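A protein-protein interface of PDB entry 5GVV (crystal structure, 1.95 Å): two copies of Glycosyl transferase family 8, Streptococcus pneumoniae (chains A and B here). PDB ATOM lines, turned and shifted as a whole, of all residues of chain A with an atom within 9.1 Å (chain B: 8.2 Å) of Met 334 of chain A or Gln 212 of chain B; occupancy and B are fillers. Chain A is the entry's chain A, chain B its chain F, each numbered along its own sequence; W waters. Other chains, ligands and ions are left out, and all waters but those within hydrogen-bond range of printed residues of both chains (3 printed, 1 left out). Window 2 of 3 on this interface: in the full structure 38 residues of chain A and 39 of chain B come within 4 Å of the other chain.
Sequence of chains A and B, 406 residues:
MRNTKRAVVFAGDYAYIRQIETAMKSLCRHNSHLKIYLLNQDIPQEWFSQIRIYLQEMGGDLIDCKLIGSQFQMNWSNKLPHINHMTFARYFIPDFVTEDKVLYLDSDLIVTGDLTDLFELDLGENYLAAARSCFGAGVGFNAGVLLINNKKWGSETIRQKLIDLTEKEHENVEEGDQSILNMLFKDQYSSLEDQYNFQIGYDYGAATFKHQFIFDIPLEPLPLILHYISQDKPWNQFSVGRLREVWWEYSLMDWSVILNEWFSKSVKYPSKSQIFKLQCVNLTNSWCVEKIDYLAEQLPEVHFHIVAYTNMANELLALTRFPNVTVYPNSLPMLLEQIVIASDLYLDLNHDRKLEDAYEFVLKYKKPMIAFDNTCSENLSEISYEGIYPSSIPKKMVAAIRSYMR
The backbone carbonyl oxygen (O) of Ala 207 of chain B sits at hydrogen-bond distance from the side-chain amino group (NZ) of Lys 210 of chain B, 3.2 Å away. The backbone carbonyl oxygen (O) of Thr 208 of chain B lies within hydrogen-bond range of the side-chain amino group (NZ) of Lys 210 of chain B (3.1 Å). O of Tyr 204 of chain B sits at hydrogen-bond distance from OG1 of Thr 208 of chain B, 2.9 Å away.
Among the printed residues, merely in contact across the chains: Ser 331 of chain A with Val 240 of chain B (3.9 Å), Leu 332 of chain A with Tyr 204 of chain B (3.5 Å), Leu 332 of chain A with Ala 207 of chain B (3.8 Å), Leu 332 of chain A with Thr 208 of chain B (3.3 Å), Met 334 of chain A with Lys 210 of chain B (3.7 Å), Met 334 of chain A with Gln 212 of chain B (3.7 Å), Met 334 of chain A with Phe 215 of chain B (3.7 Å), Leu 335 of chain A with Ala 207 of chain B (3.9 Å), Leu 335 of chain A with Phe 215 of chain B (3.6 Å), Leu 335 of chain A with Val 240 of chain B (3.7 Å) and Gln 338 of chain A with Phe 215 of chain B (3.8 Å).
Of chain B, only Lys 210, Gln 212 and Phe 215 come within 4 Å of Met 334 of chain A. Of the printed residues of chain B, Leu 335 of chain A touches Ala 207 (3.9 Å), Phe 215 (3.6 Å) and Val 240 (3.7 Å). Ile 341 of chain A touches none of the printed residues of chain B. Asp 357 of chain A touches none of the printed residues of chain B. Of the printed residues of chain A, Lys 210 of chain B touches Met 334 (3.7 Å). Gln 212 of chain B touches just one residue of chain A: Met 334 (3.7 Å). Phe 213 of chain B touches none of the printed residues of chain A.
Hydrophobic or aromatic side chains of chain B that line the printed part of chain A: Tyr 204, Ala 207, Phe 215 and Val 240. Of the 17 printed residues of chain A, 5 touch a printed residue of chain B. Among the printed residues, no Asp or Glu carboxylate lies within 4 Å of a Lys or Arg side-chain nitrogen of the other chain.
No position is printed for both chains. Of the 11 pairs that touch across the chains among the printed residues, none has its exchanged pair printed and touching as well.
Water W2 lies within hydrogen-bond range of OG of Ser 331 of chain A and O of Val 240 of chain B. Water W3 lies within hydrogen-bond range of OE1 of Gln 338 of chain A (2.9 Å) and NH1 of Arg 242 of chain B (3.0 Å). Water W1 lies within hydrogen-bond range of the backbone carbonyl oxygen of Ala 207 of chain B and the backbone NH of Met 334 of chain A.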
ATOM      1  N   LEU A 283     -12.809   5.974 -19.315  1.00  0.00           N
ATOM      2  CA  LEU A 283     -12.422   7.366 -19.489  1.00  0.00           C
ATOM      3  C   LEU A 283     -13.683   8.208 -19.381  1.00  0.00           C
ATOM      4  O   LEU A 283     -14.624   8.026 -20.158  1.00  0.00           O
ATOM      5  CB  LEU A 283     -11.774   7.566 -20.864  1.00  0.00           C
ATOM      6  CG  LEU A 283     -11.539   8.993 -21.361  1.00  0.00           C
ATOM      7  CD1 LEU A 283     -10.358   9.643 -20.659  1.00  0.00           C
ATOM      8  CD2 LEU A 283     -11.326   9.002 -22.870  1.00  0.00           C
ATOM      9  N   VAL A 307     -10.072   7.305 -15.620  1.00  0.00           N
ATOM     10  CA  VAL A 307      -9.213   8.351 -16.162  1.00  0.00           C
ATOM     11  C   VAL A 307     -10.059   9.543 -16.591  1.00  0.00           C
ATOM     12  O   VAL A 307     -11.184   9.373 -17.053  1.00  0.00           O
ATOM     13  CB  VAL A 307      -8.419   7.808 -17.367  1.00  0.00           C
ATOM     14  CG1 VAL A 307      -7.417   8.831 -17.878  1.00  0.00           C
ATOM     15  CG2 VAL A 307      -7.700   6.521 -16.980  1.00  0.00           C
ATOM     16  N   TYR A 309      -9.437  13.793 -18.338  1.00  0.00           N
ATOM     17  CA  TYR A 309      -8.476  14.724 -18.919  1.00  0.00           C
ATOM     18  C   TYR A 309      -8.524  16.058 -18.178  1.00  0.00           C
ATOM     19  O   TYR A 309      -7.899  17.032 -18.593  1.00  0.00           O
ATOM     20  CB  TYR A 309      -8.794  14.963 -20.402  1.00  0.00           C
ATOM     21  CG  TYR A 309      -8.551  13.777 -21.321  1.00  0.00           C
ATOM     22  CD1 TYR A 309      -7.752  12.710 -20.927  1.00  0.00           C
ATOM     23  CD2 TYR A 309      -9.126  13.732 -22.590  1.00  0.00           C
ATOM     24  CE1 TYR A 309      -7.531  11.629 -21.774  1.00  0.00           C
ATOM     25  CE2 TYR A 309      -8.910  12.656 -23.440  1.00  0.00           C
ATOM     26  CZ  TYR A 309      -8.114  11.610 -23.027  1.00  0.00           C
ATOM     27  OH  TYR A 309      -7.896  10.543 -23.875  1.00  0.00           O
ATOM     28  N   SER A 331      -5.297  13.761 -16.696  1.00  0.00           N
ATOM     29  CA  SER A 331      -4.431  12.922 -17.516  1.00  0.00           C
ATOM     30  C   SER A 331      -4.517  13.412 -18.959  1.00  0.00           C
ATOM     31  O   SER A 331      -5.135  14.449 -19.232  1.00  0.00           O
ATOM     32  CB  SER A 331      -4.853  11.458 -17.401  1.00  0.00           C
ATOM     33  OG  SER A 331      -3.889  10.591 -17.969  1.00  0.00           O
ATOM     34  N   LEU A 332      -3.891  12.684 -19.878  1.00  0.00           N
ATOM     35  CA  LEU A 332      -3.869  13.080 -21.287  1.00  0.00           C
ATOM     36  C   LEU A 332      -3.973  11.832 -22.173  1.00  0.00           C
ATOM     37  O   LEU A 332      -3.714  10.723 -21.702  1.00  0.00           O
ATOM     38  CB  LEU A 332      -2.596  13.885 -21.590  1.00  0.00           C
ATOM     39  CG  LEU A 332      -2.475  15.269 -20.936  1.00  0.00           C
ATOM     40  CD1 LEU A 332      -1.036  15.765 -20.930  1.00  0.00           C
ATOM     41  CD2 LEU A 332      -3.367  16.279 -21.633  1.00  0.00           C
ATOM     42  N   PRO A 333      -4.376  12.004 -23.446  1.00  0.00           N
ATOM     43  CA  PRO A 333      -4.591  10.860 -24.346  1.00  0.00           C
ATOM     44  C   PRO A 333      -3.445   9.840 -24.429  1.00  0.00           C
ATOM     45  O   PRO A 333      -3.732   8.644 -24.462  1.00  0.00           O
ATOM     46  CB  PRO A 333      -4.798  11.528 -25.705  1.00  0.00           C
ATOM     47  CG  PRO A 333      -5.476  12.820 -25.361  1.00  0.00           C
ATOM     48  CD  PRO A 333      -4.835  13.269 -24.056  1.00  0.00           C
ATOM     49  N   MET A 334      -2.184  10.267 -24.431  1.00  0.00           N
ATOM     50  CA  MET A 334      -1.071   9.311 -24.516  1.00  0.00           C
ATOM     51  C   MET A 334      -0.952   8.461 -23.279  1.00  0.00           C
ATOM     52  O   MET A 334      -0.505   7.324 -23.315  1.00  0.00           O
ATOM     53  CB  MET A 334       0.193  10.072 -24.891  1.00  0.00           C
ATOM     54  CG  MET A 334       0.174  10.368 -26.392  1.00  0.00           C
ATOM     55  SD  MET A 334       1.744  11.504 -26.875  1.00  0.00           S
ATOM     56  CE  MET A 334       1.063  11.953 -28.711  1.00  0.00           C
ATOM     57  N   LEU A 335      -1.389   9.023 -22.174  1.00  0.00           N
ATOM     58  CA  LEU A 335      -1.347   8.294 -20.905  1.00  0.00           C
ATOM     59  C   LEU A 335      -2.519   7.316 -20.800  1.00  0.00           C
ATOM     60  O   LEU A 335      -2.352   6.178 -20.353  1.00  0.00           O
ATOM     61  CB  LEU A 335      -1.345   9.275 -19.728  1.00  0.00           C
ATOM     62  CG  LEU A 335      -0.242  10.337 -19.841  1.00  0.00           C
ATOM     63  CD1 LEU A 335      -0.355  11.407 -18.761  1.00  0.00           C
ATOM     64  CD2 LEU A 335       1.122   9.680 -19.790  1.00  0.00           C
ATOM     65  N   LEU A 336      -3.703   7.763 -21.215  1.00  0.00           N
ATOM     66  CA  LEU A 336      -4.874   6.892 -21.284  1.00  0.00           C
ATOM     67  C   LEU A 336      -4.601   5.709 -22.216  1.00  0.00           C
ATOM     68  O   LEU A 336      -4.974   4.575 -21.911  1.00  0.00           O
ATOM     69  CB  LEU A 336      -6.096   7.690 -21.759  1.00  0.00           C
ATOM     70  CG  LEU A 336      -7.503   7.076 -21.838  1.00  0.00           C
ATOM     71  CD1 LEU A 336      -7.867   6.683 -23.256  1.00  0.00           C
ATOM     72  CD2 LEU A 336      -7.692   5.895 -20.879  1.00  0.00           C
ATOM     73  N   GLU A 337      -3.939   5.964 -23.344  1.00  0.00           N
ATOM     74  CA  GLU A 337      -3.634   4.891 -24.291  1.00  0.00           C
ATOM     75  C   GLU A 337      -2.812   3.774 -23.642  1.00  0.00           C
ATOM     76  O   GLU A 337      -3.072   2.590 -23.883  1.00  0.00           O
ATOM     77  CB  GLU A 337      -2.909   5.429 -25.533  1.00  0.00           C
ATOM     78  CG  GLU A 337      -2.472   4.328 -26.503  1.00  0.00           C
ATOM     79  CD  GLU A 337      -1.939   4.855 -27.826  1.00  0.00           C
ATOM     80  OE1 GLU A 337      -1.283   5.920 -27.841  1.00  0.00           O
ATOM     81  OE2 GLU A 337      -2.169   4.184 -28.852  1.00  0.00           O
ATOM     82  N   GLN A 338      -1.830   4.144 -22.819  1.00  0.00           N
ATOM     83  CA  GLN A 338      -0.977   3.149 -22.175  1.00  0.00           C
ATOM     84  C   GLN A 338      -1.750   2.333 -21.143  1.00  0.00           C
ATOM     85  O   GLN A 338      -1.486   1.142 -20.958  1.00  0.00           O
ATOM     86  CB  GLN A 338       0.247   3.808 -21.527  1.00  0.00           C
ATOM     87  CG  GLN A 338       1.204   4.460 -22.528  1.00  0.00           C
ATOM     88  CD  GLN A 338       1.601   3.514 -23.648  1.00  0.00           C
ATOM     89  OE1 GLN A 338       2.060   2.400 -23.398  1.00  0.00           O
ATOM     90  NE2 GLN A 338       1.411   3.947 -24.890  1.00  0.00           N
ATOM     91  N   ILE A 339      -2.700   2.975 -20.469  1.00  0.00           N
ATOM     92  CA  ILE A 339      -3.555   2.281 -19.506  1.00  0.00           C
ATOM     93  C   ILE A 339      -4.477   1.291 -20.223  1.00  0.00           C
ATOM     94  O   ILE A 339      -4.691   0.176 -19.742  1.00  0.00           O
ATOM     95  CB  ILE A 339      -4.377   3.273 -18.648  1.00  0.00           C
ATOM     96  CG1 ILE A 339      -3.435   4.152 -17.822  1.00  0.00           C
ATOM     97  CG2 ILE A 339      -5.347   2.533 -17.719  1.00  0.00           C
ATOM     98  CD1 ILE A 339      -4.121   5.271 -17.046  1.00  0.00           C
ATOM     99  N   VAL A 340      -5.010   1.692 -21.374  1.00  0.00           N
ATOM    100  CA  VAL A 340      -5.873   0.808 -22.156  1.00  0.00           C
ATOM    101  C   VAL A 340      -5.122  -0.452 -22.597  1.00  0.00           C
ATOM    102  O   VAL A 340      -5.618  -1.567 -22.423  1.00  0.00           O
ATOM    103  CB  VAL A 340      -6.477   1.529 -23.380  1.00  0.00           C
ATOM    104  CG1 VAL A 340      -7.290   0.555 -24.222  1.00  0.00           C
ATOM    105  CG2 VAL A 340      -7.364   2.684 -22.926  1.00  0.00           C
ATOM    106  N   ILE A 341      -3.926  -0.275 -23.152  1.00  0.00           N
ATOM    107  CA  ILE A 341      -3.073  -1.401 -23.539  1.00  0.00           C
ATOM    108  C   ILE A 341      -2.865  -2.369 -22.373  1.00  0.00           C
ATOM    109  O   ILE A 341      -2.832  -3.586 -22.555  1.00  0.00           O
ATOM    110  CB  ILE A 341      -1.697  -0.904 -24.040  1.00  0.00           C
ATOM    111  CG1 ILE A 341      -1.854  -0.072 -25.316  1.00  0.00           C
ATOM    112  CG2 ILE A 341      -0.741  -2.067 -24.285  1.00  0.00           C
ATOM    113  CD1 ILE A 341      -0.548   0.543 -25.799  1.00  0.00           C
ATOM    114  N   ASP A 357     -11.693   8.348 -29.528  1.00  0.00           N
ATOM    115  CA  ASP A 357     -10.382   7.688 -29.570  1.00  0.00           C
ATOM    116  C   ASP A 357     -10.181   6.569 -28.541  1.00  0.00           C
ATOM    117  O   ASP A 357      -9.365   5.671 -28.749  1.00  0.00           O
ATOM    118  CB  ASP A 357      -9.237   8.705 -29.476  1.00  0.00           C
ATOM    119  CG  ASP A 357      -8.657   9.056 -30.839  1.00  0.00           C
ATOM    120  OD1 ASP A 357      -9.024   8.394 -31.837  1.00  0.00           O
ATOM    121  OD2 ASP A 357      -7.826   9.987 -30.912  1.00  0.00           O
ATOM    122  N   PHE A 361      -8.652   3.124 -29.402  1.00  0.00           N
ATOM    123  CA  PHE A 361      -7.664   2.364 -28.648  1.00  0.00           C
ATOM    124  C   PHE A 361      -8.221   0.980 -28.332  1.00  0.00           C
ATOM    125  O   PHE A 361      -7.514  -0.020 -28.449  1.00  0.00           O
ATOM    126  CB  PHE A 361      -7.284   3.091 -27.352  1.00  0.00           C
ATOM    127  CG  PHE A 361      -6.663   4.445 -27.567  1.00  0.00           C
ATOM    128  CD1 PHE A 361      -6.020   4.757 -28.762  1.00  0.00           C
ATOM    129  CD2 PHE A 361      -6.723   5.411 -26.571  1.00  0.00           C
ATOM    130  CE1 PHE A 361      -5.448   6.006 -28.954  1.00  0.00           C
ATOM    131  CE2 PHE A 361      -6.156   6.661 -26.758  1.00  0.00           C
ATOM    132  CZ  PHE A 361      -5.521   6.960 -27.949  1.00  0.00           C
ATOM    133  N   TYR A 365      -6.323  -2.382 -29.894  1.00  0.00           N
ATOM    134  CA  TYR A 365      -5.648  -3.335 -29.020  1.00  0.00           C
ATOM    135  C   TYR A 365      -6.532  -4.545 -28.671  1.00  0.00           C
ATOM    136  O   TYR A 365      -6.226  -5.315 -27.756  1.00  0.00           O
ATOM    137  CB  TYR A 365      -5.103  -2.614 -27.780  1.00  0.00           C
ATOM    138  CG  TYR A 365      -4.156  -1.477 -28.143  1.00  0.00           C
ATOM    139  CD1 TYR A 365      -2.906  -1.738 -28.687  1.00  0.00           C
ATOM    140  CD2 TYR A 365      -4.519  -0.146 -27.947  1.00  0.00           C
ATOM    141  CE1 TYR A 365      -2.041  -0.710 -29.029  1.00  0.00           C
ATOM    142  CE2 TYR A 365      -3.661   0.890 -28.282  1.00  0.00           C
ATOM    143  CZ  TYR A 365      -2.423   0.601 -28.825  1.00  0.00           C
ATOM    144  OH  TYR A 365      -1.565   1.628 -29.158  1.00  0.00           O
ATOM    145  N   ASP B 203       6.820  11.827 -18.414  1.00  0.00           N
ATOM    146  CA  ASP B 203       5.587  11.292 -19.010  1.00  0.00           C
ATOM    147  C   ASP B 203       4.516  12.356 -19.288  1.00  0.00           C
ATOM    148  O   ASP B 203       3.982  12.428 -20.400  1.00  0.00           O
ATOM    149  CB  ASP B 203       4.996  10.186 -18.131  1.00  0.00           C
ATOM    150  CG  ASP B 203       5.631   8.835 -18.387  1.00  0.00           C
ATOM    151  OD1 ASP B 203       6.619   8.768 -19.150  1.00  0.00           O
ATOM    152  OD2 ASP B 203       5.145   7.835 -17.814  1.00  0.00           O
ATOM    153  N   TYR B 204       4.217  13.184 -18.288  1.00  0.00           N
ATOM    154  CA  TYR B 204       3.202  14.228 -18.445  1.00  0.00           C
ATOM    155  C   TYR B 204       3.630  15.253 -19.488  1.00  0.00           C
ATOM    156  O   TYR B 204       2.834  15.639 -20.351  1.00  0.00           O
ATOM    157  CB  TYR B 204       2.918  14.920 -17.109  1.00  0.00           C
ATOM    158  CG  TYR B 204       1.644  15.740 -17.092  1.00  0.00           C
ATOM    159  CD1 TYR B 204       0.427  15.173 -17.444  1.00  0.00           C
ATOM    160  CD2 TYR B 204       1.655  17.075 -16.704  1.00  0.00           C
ATOM    161  CE1 TYR B 204      -0.740  15.911 -17.427  1.00  0.00           C
ATOM    162  CE2 TYR B 204       0.488  17.825 -16.679  1.00  0.00           C
ATOM    163  CZ  TYR B 204      -0.706  17.234 -17.042  1.00  0.00           C
ATOM    164  OH  TYR B 204      -1.877  17.961 -17.025  1.00  0.00           O
ATOM    165  N   GLY B 205       4.887  15.689 -19.412  1.00  0.00           N
ATOM    166  CA  GLY B 205       5.437  16.598 -20.402  1.00  0.00           C
ATOM    167  C   GLY B 205       5.367  16.048 -21.816  1.00  0.00           C
ATOM    168  O   GLY B 205       4.947  16.743 -22.742  1.00  0.00           O
ATOM    169  N   ALA B 206       5.767  14.792 -21.982  1.00  0.00           N
ATOM    170  CA  ALA B 206       5.753  14.152 -23.294  1.00  0.00           C
ATOM    171  C   ALA B 206       4.336  14.101 -23.845  1.00  0.00           C
ATOM    172  O   ALA B 206       4.092  14.415 -25.011  1.00  0.00           O
ATOM    173  CB  ALA B 206       6.332  12.750 -23.200  1.00  0.00           C
ATOM    174  N   ALA B 207       3.405  13.693 -22.993  1.00  0.00           N
ATOM    175  CA  ALA B 207       1.996  13.635 -23.355  1.00  0.00           C
ATOM    176  C   ALA B 207       1.446  15.022 -23.688  1.00  0.00           C
ATOM    177  O   ALA B 207       0.526  15.156 -24.504  1.00  0.00           O
ATOM    178  CB  ALA B 207       1.201  13.007 -22.214  1.00  0.00           C
ATOM    179  N   THR B 208       1.989  16.040 -23.024  1.00  0.00           N
ATOM    180  CA  THR B 208       1.566  17.426 -23.214  1.00  0.00           C
ATOM    181  C   THR B 208       2.057  17.970 -24.554  1.00  0.00           C
ATOM    182  O   THR B 208       1.284  18.559 -25.316  1.00  0.00           O
ATOM    183  CB  THR B 208       2.088  18.336 -22.080  1.00  0.00           C
ATOM    184  OG1 THR B 208       1.341  18.095 -20.880  1.00  0.00           O
ATOM    185  CG2 THR B 208       1.941  19.799 -22.455  1.00  0.00           C
ATOM    186  N   PHE B 209       3.341  17.780 -24.839  1.00  0.00           N
ATOM    187  CA  PHE B 209       3.913  18.304 -26.073  1.00  0.00           C
ATOM    188  C   PHE B 209       3.782  17.316 -27.238  1.00  0.00           C
ATOM    189  O   PHE B 209       4.268  17.579 -28.342  1.00  0.00           O
ATOM    190  CB  PHE B 209       5.364  18.742 -25.844  1.00  0.00           C
ATOM    191  CG  PHE B 209       5.509  19.804 -24.784  1.00  0.00           C
ATOM    192  CD1 PHE B 209       5.201  21.131 -25.066  1.00  0.00           C
ATOM    193  CD2 PHE B 209       5.944  19.476 -23.508  1.00  0.00           C
ATOM    194  CE1 PHE B 209       5.322  22.109 -24.089  1.00  0.00           C
ATOM    195  CE2 PHE B 209       6.071  20.448 -22.527  1.00  0.00           C
ATOM    196  CZ  PHE B 209       5.761  21.766 -22.819  1.00  0.00           C
ATOM    197  N   LYS B 210       3.109  16.194 -26.977  1.00  0.00           N
ATOM    198  CA  LYS B 210       2.809  15.169 -27.985  1.00  0.00           C
ATOM    199  C   LYS B 210       4.032  14.441 -28.533  1.00  0.00           C
ATOM    200  O   LYS B 210       4.135  14.206 -29.741  1.00  0.00           O
ATOM    201  CB  LYS B 210       1.968  15.727 -29.145  1.00  0.00           C
ATOM    202  CG  LYS B 210       0.471  15.714 -28.892  1.00  0.00           C
ATOM    203  CD  LYS B 210       0.075  16.768 -27.893  1.00  0.00           C
ATOM    204  CE  LYS B 210      -1.178  16.354 -27.137  1.00  0.00           C
ATOM    205  NZ  LYS B 210      -1.403  17.245 -25.966  1.00  0.00           N
ATOM    206  N   HIS B 211       4.946  14.071 -27.645  1.00  0.00           N
ATOM    207  CA  HIS B 211       6.093  13.275 -28.047  1.00  0.00           C
ATOM    208  C   HIS B 211       5.708  11.801 -27.964  1.00  0.00           C
ATOM    209  O   HIS B 211       5.965  11.133 -26.967  1.00  0.00           O
ATOM    210  CB  HIS B 211       7.307  13.622 -27.177  1.00  0.00           C
ATOM    211  CG  HIS B 211       7.744  15.047 -27.310  1.00  0.00           C
ATOM    212  ND1 HIS B 211       8.279  15.771 -26.262  1.00  0.00           N
ATOM    213  CD2 HIS B 211       7.725  15.893 -28.370  1.00  0.00           C
ATOM    214  CE1 HIS B 211       8.570  16.990 -26.671  1.00  0.00           C
ATOM    215  NE2 HIS B 211       8.242  17.093 -27.947  1.00  0.00           N
ATOM    216  N   GLN B 212       5.075  11.306 -29.026  1.00  0.00           N
ATOM    217  CA  GLN B 212       4.438   9.989 -29.024  1.00  0.00           C
ATOM    218  C   GLN B 212       5.400   8.811 -28.816  1.00  0.00           C
ATOM    219  O   GLN B 212       5.032   7.790 -28.221  1.00  0.00           O
ATOM    220  CB  GLN B 212       3.646   9.799 -30.323  1.00  0.00           C
ATOM    221  CG  GLN B 212       4.473  10.048 -31.586  1.00  0.00           C
ATOM    222  CD  GLN B 212       3.654   9.969 -32.863  1.00  0.00           C
ATOM    223  OE1 GLN B 212       3.784  10.816 -33.749  1.00  0.00           O
ATOM    224  NE2 GLN B 212       2.826   8.938 -32.975  1.00  0.00           N
ATOM    225  N   PHE B 213       6.627   8.949 -29.302  1.00  0.00           N
ATOM    226  CA  PHE B 213       7.565   7.831 -29.294  1.00  0.00           C
ATOM    227  C   PHE B 213       8.239   7.585 -27.939  1.00  0.00           C
ATOM    228  O   PHE B 213       8.794   6.508 -27.702  1.00  0.00           O
ATOM    229  CB  PHE B 213       8.590   8.009 -30.414  1.00  0.00           C
ATOM    230  CG  PHE B 213       7.970   8.015 -31.787  1.00  0.00           C
ATOM    231  CD1 PHE B 213       7.506   6.834 -32.350  1.00  0.00           C
ATOM    232  CD2 PHE B 213       7.834   9.197 -32.505  1.00  0.00           C
ATOM    233  CE1 PHE B 213       6.926   6.821 -33.611  1.00  0.00           C
ATOM    234  CE2 PHE B 213       7.255   9.199 -33.775  1.00  0.00           C
ATOM    235  CZ  PHE B 213       6.800   8.009 -34.327  1.00  0.00           C
ATOM    236  N   ILE B 214       8.176   8.573 -27.051  1.00  0.00           N
ATOM    237  CA  ILE B 214       8.593   8.385 -25.657  1.00  0.00           C
ATOM    238  C   ILE B 214       7.954   7.134 -25.044  1.00  0.00           C
ATOM    239  O   ILE B 214       8.595   6.391 -24.293  1.00  0.00           O
ATOM    240  CB  ILE B 214       8.198   9.596 -24.788  1.00  0.00           C
ATOM    241  CG1 ILE B 214       8.896  10.865 -25.271  1.00  0.00           C
ATOM    242  CG2 ILE B 214       8.550   9.349 -23.321  1.00  0.00           C
ATOM    243  CD1 ILE B 214      10.357  10.931 -24.865  1.00  0.00           C
ATOM    244  N   PHE B 215       6.687   6.899 -25.378  1.00  0.00           N
ATOM    245  CA  PHE B 215       5.930   5.827 -24.741  1.00  0.00           C
ATOM    246  C   PHE B 215       6.187   4.454 -25.365  1.00  0.00           C
ATOM    247  O   PHE B 215       5.606   3.451 -24.931  1.00  0.00           O
ATOM    248  CB  PHE B 215       4.437   6.178 -24.717  1.00  0.00           C
ATOM    249  CG  PHE B 215       4.145   7.477 -24.014  1.00  0.00           C
ATOM    250  CD1 PHE B 215       4.004   7.515 -22.631  1.00  0.00           C
ATOM    251  CD2 PHE B 215       4.044   8.663 -24.730  1.00  0.00           C
ATOM    252  CE1 PHE B 215       3.757   8.715 -21.974  1.00  0.00           C
ATOM    253  CE2 PHE B 215       3.797   9.866 -24.084  1.00  0.00           C
ATOM    254  CZ  PHE B 215       3.651   9.892 -22.704  1.00  0.00           C
ATOM    255  N   ASP B 216       7.068   4.411 -26.365  1.00  0.00           N
ATOM    256  CA  ASP B 216       7.477   3.151 -26.990  1.00  0.00           C
ATOM    257  C   ASP B 216       8.786   2.620 -26.391  1.00  0.00           C
ATOM    258  O   ASP B 216       9.166   1.468 -26.618  1.00  0.00           O
ATOM    259  CB  ASP B 216       7.619   3.310 -28.511  1.00  0.00           C
ATOM    260  CG  ASP B 216       6.285   3.548 -29.207  1.00  0.00           C
ATOM    261  OD1 ASP B 216       5.230   3.197 -28.631  1.00  0.00           O
ATOM    262  OD2 ASP B 216       6.290   4.082 -30.340  1.00  0.00           O
ATOM    263  N   ILE B 217       9.473   3.465 -25.628  1.00  0.00           N
ATOM    264  CA  ILE B 217      10.712   3.065 -24.971  1.00  0.00           C
ATOM    265  C   ILE B 217      10.415   1.981 -23.937  1.00  0.00           C
ATOM    266  O   ILE B 217       9.566   2.170 -23.063  1.00  0.00           O
ATOM    267  CB  ILE B 217      11.395   4.263 -24.279  1.00  0.00           C
ATOM    268  CG1 ILE B 217      11.626   5.404 -25.274  1.00  0.00           C
ATOM    269  CG2 ILE B 217      12.707   3.836 -23.638  1.00  0.00           C
ATOM    270  CD1 ILE B 217      12.115   6.703 -24.619  1.00  0.00           C
ATOM    271  N   VAL B 240      -0.054  10.911 -12.822  1.00  0.00           N
ATOM    272  CA  VAL B 240      -0.461  10.305 -14.090  1.00  0.00           C
ATOM    273  C   VAL B 240       0.693   9.620 -14.830  1.00  0.00           C
ATOM    274  O   VAL B 240       0.470   8.878 -15.789  1.00  0.00           O
ATOM    275  CB  VAL B 240      -1.146  11.330 -15.012  1.00  0.00           C
ATOM    276  CG1 VAL B 240      -2.454  11.810 -14.396  1.00  0.00           C
ATOM    277  CG2 VAL B 240      -0.221  12.506 -15.271  1.00  0.00           C
ATOM    278  N   ARG B 242       3.928   6.996 -15.455  1.00  0.00           N
ATOM    279  CA  ARG B 242       4.076   5.551 -15.248  1.00  0.00           C
ATOM    280  C   ARG B 242       5.087   5.196 -14.155  1.00  0.00           C
ATOM    281  O   ARG B 242       5.860   6.056 -13.704  1.00  0.00           O
ATOM    282  CB  ARG B 242       4.471   4.864 -16.561  1.00  0.00           C
ATOM    283  CG  ARG B 242       3.401   4.940 -17.658  1.00  0.00           C
ATOM    284  CD  ARG B 242       3.983   4.614 -19.025  1.00  0.00           C
ATOM    285  NE  ARG B 242       5.068   5.529 -19.365  1.00  0.00           N
ATOM    286  CZ  ARG B 242       5.915   5.345 -20.373  1.00  0.00           C
ATOM    287  NH1 ARG B 242       5.797   4.279 -21.154  1.00  0.00           N
ATOM    288  NH2 ARG B 242       6.878   6.229 -20.608  1.00  0.00           N
HETATM  289  O   HOH W   1      -1.553  13.145 -25.082  1.00  0.00           O
HETATM  290  O   HOH W   2      -2.988   8.686 -16.288  1.00  0.00           O
HETATM  291  O   HOH W   3       3.942   1.974 -21.215  1.00  0.00           O
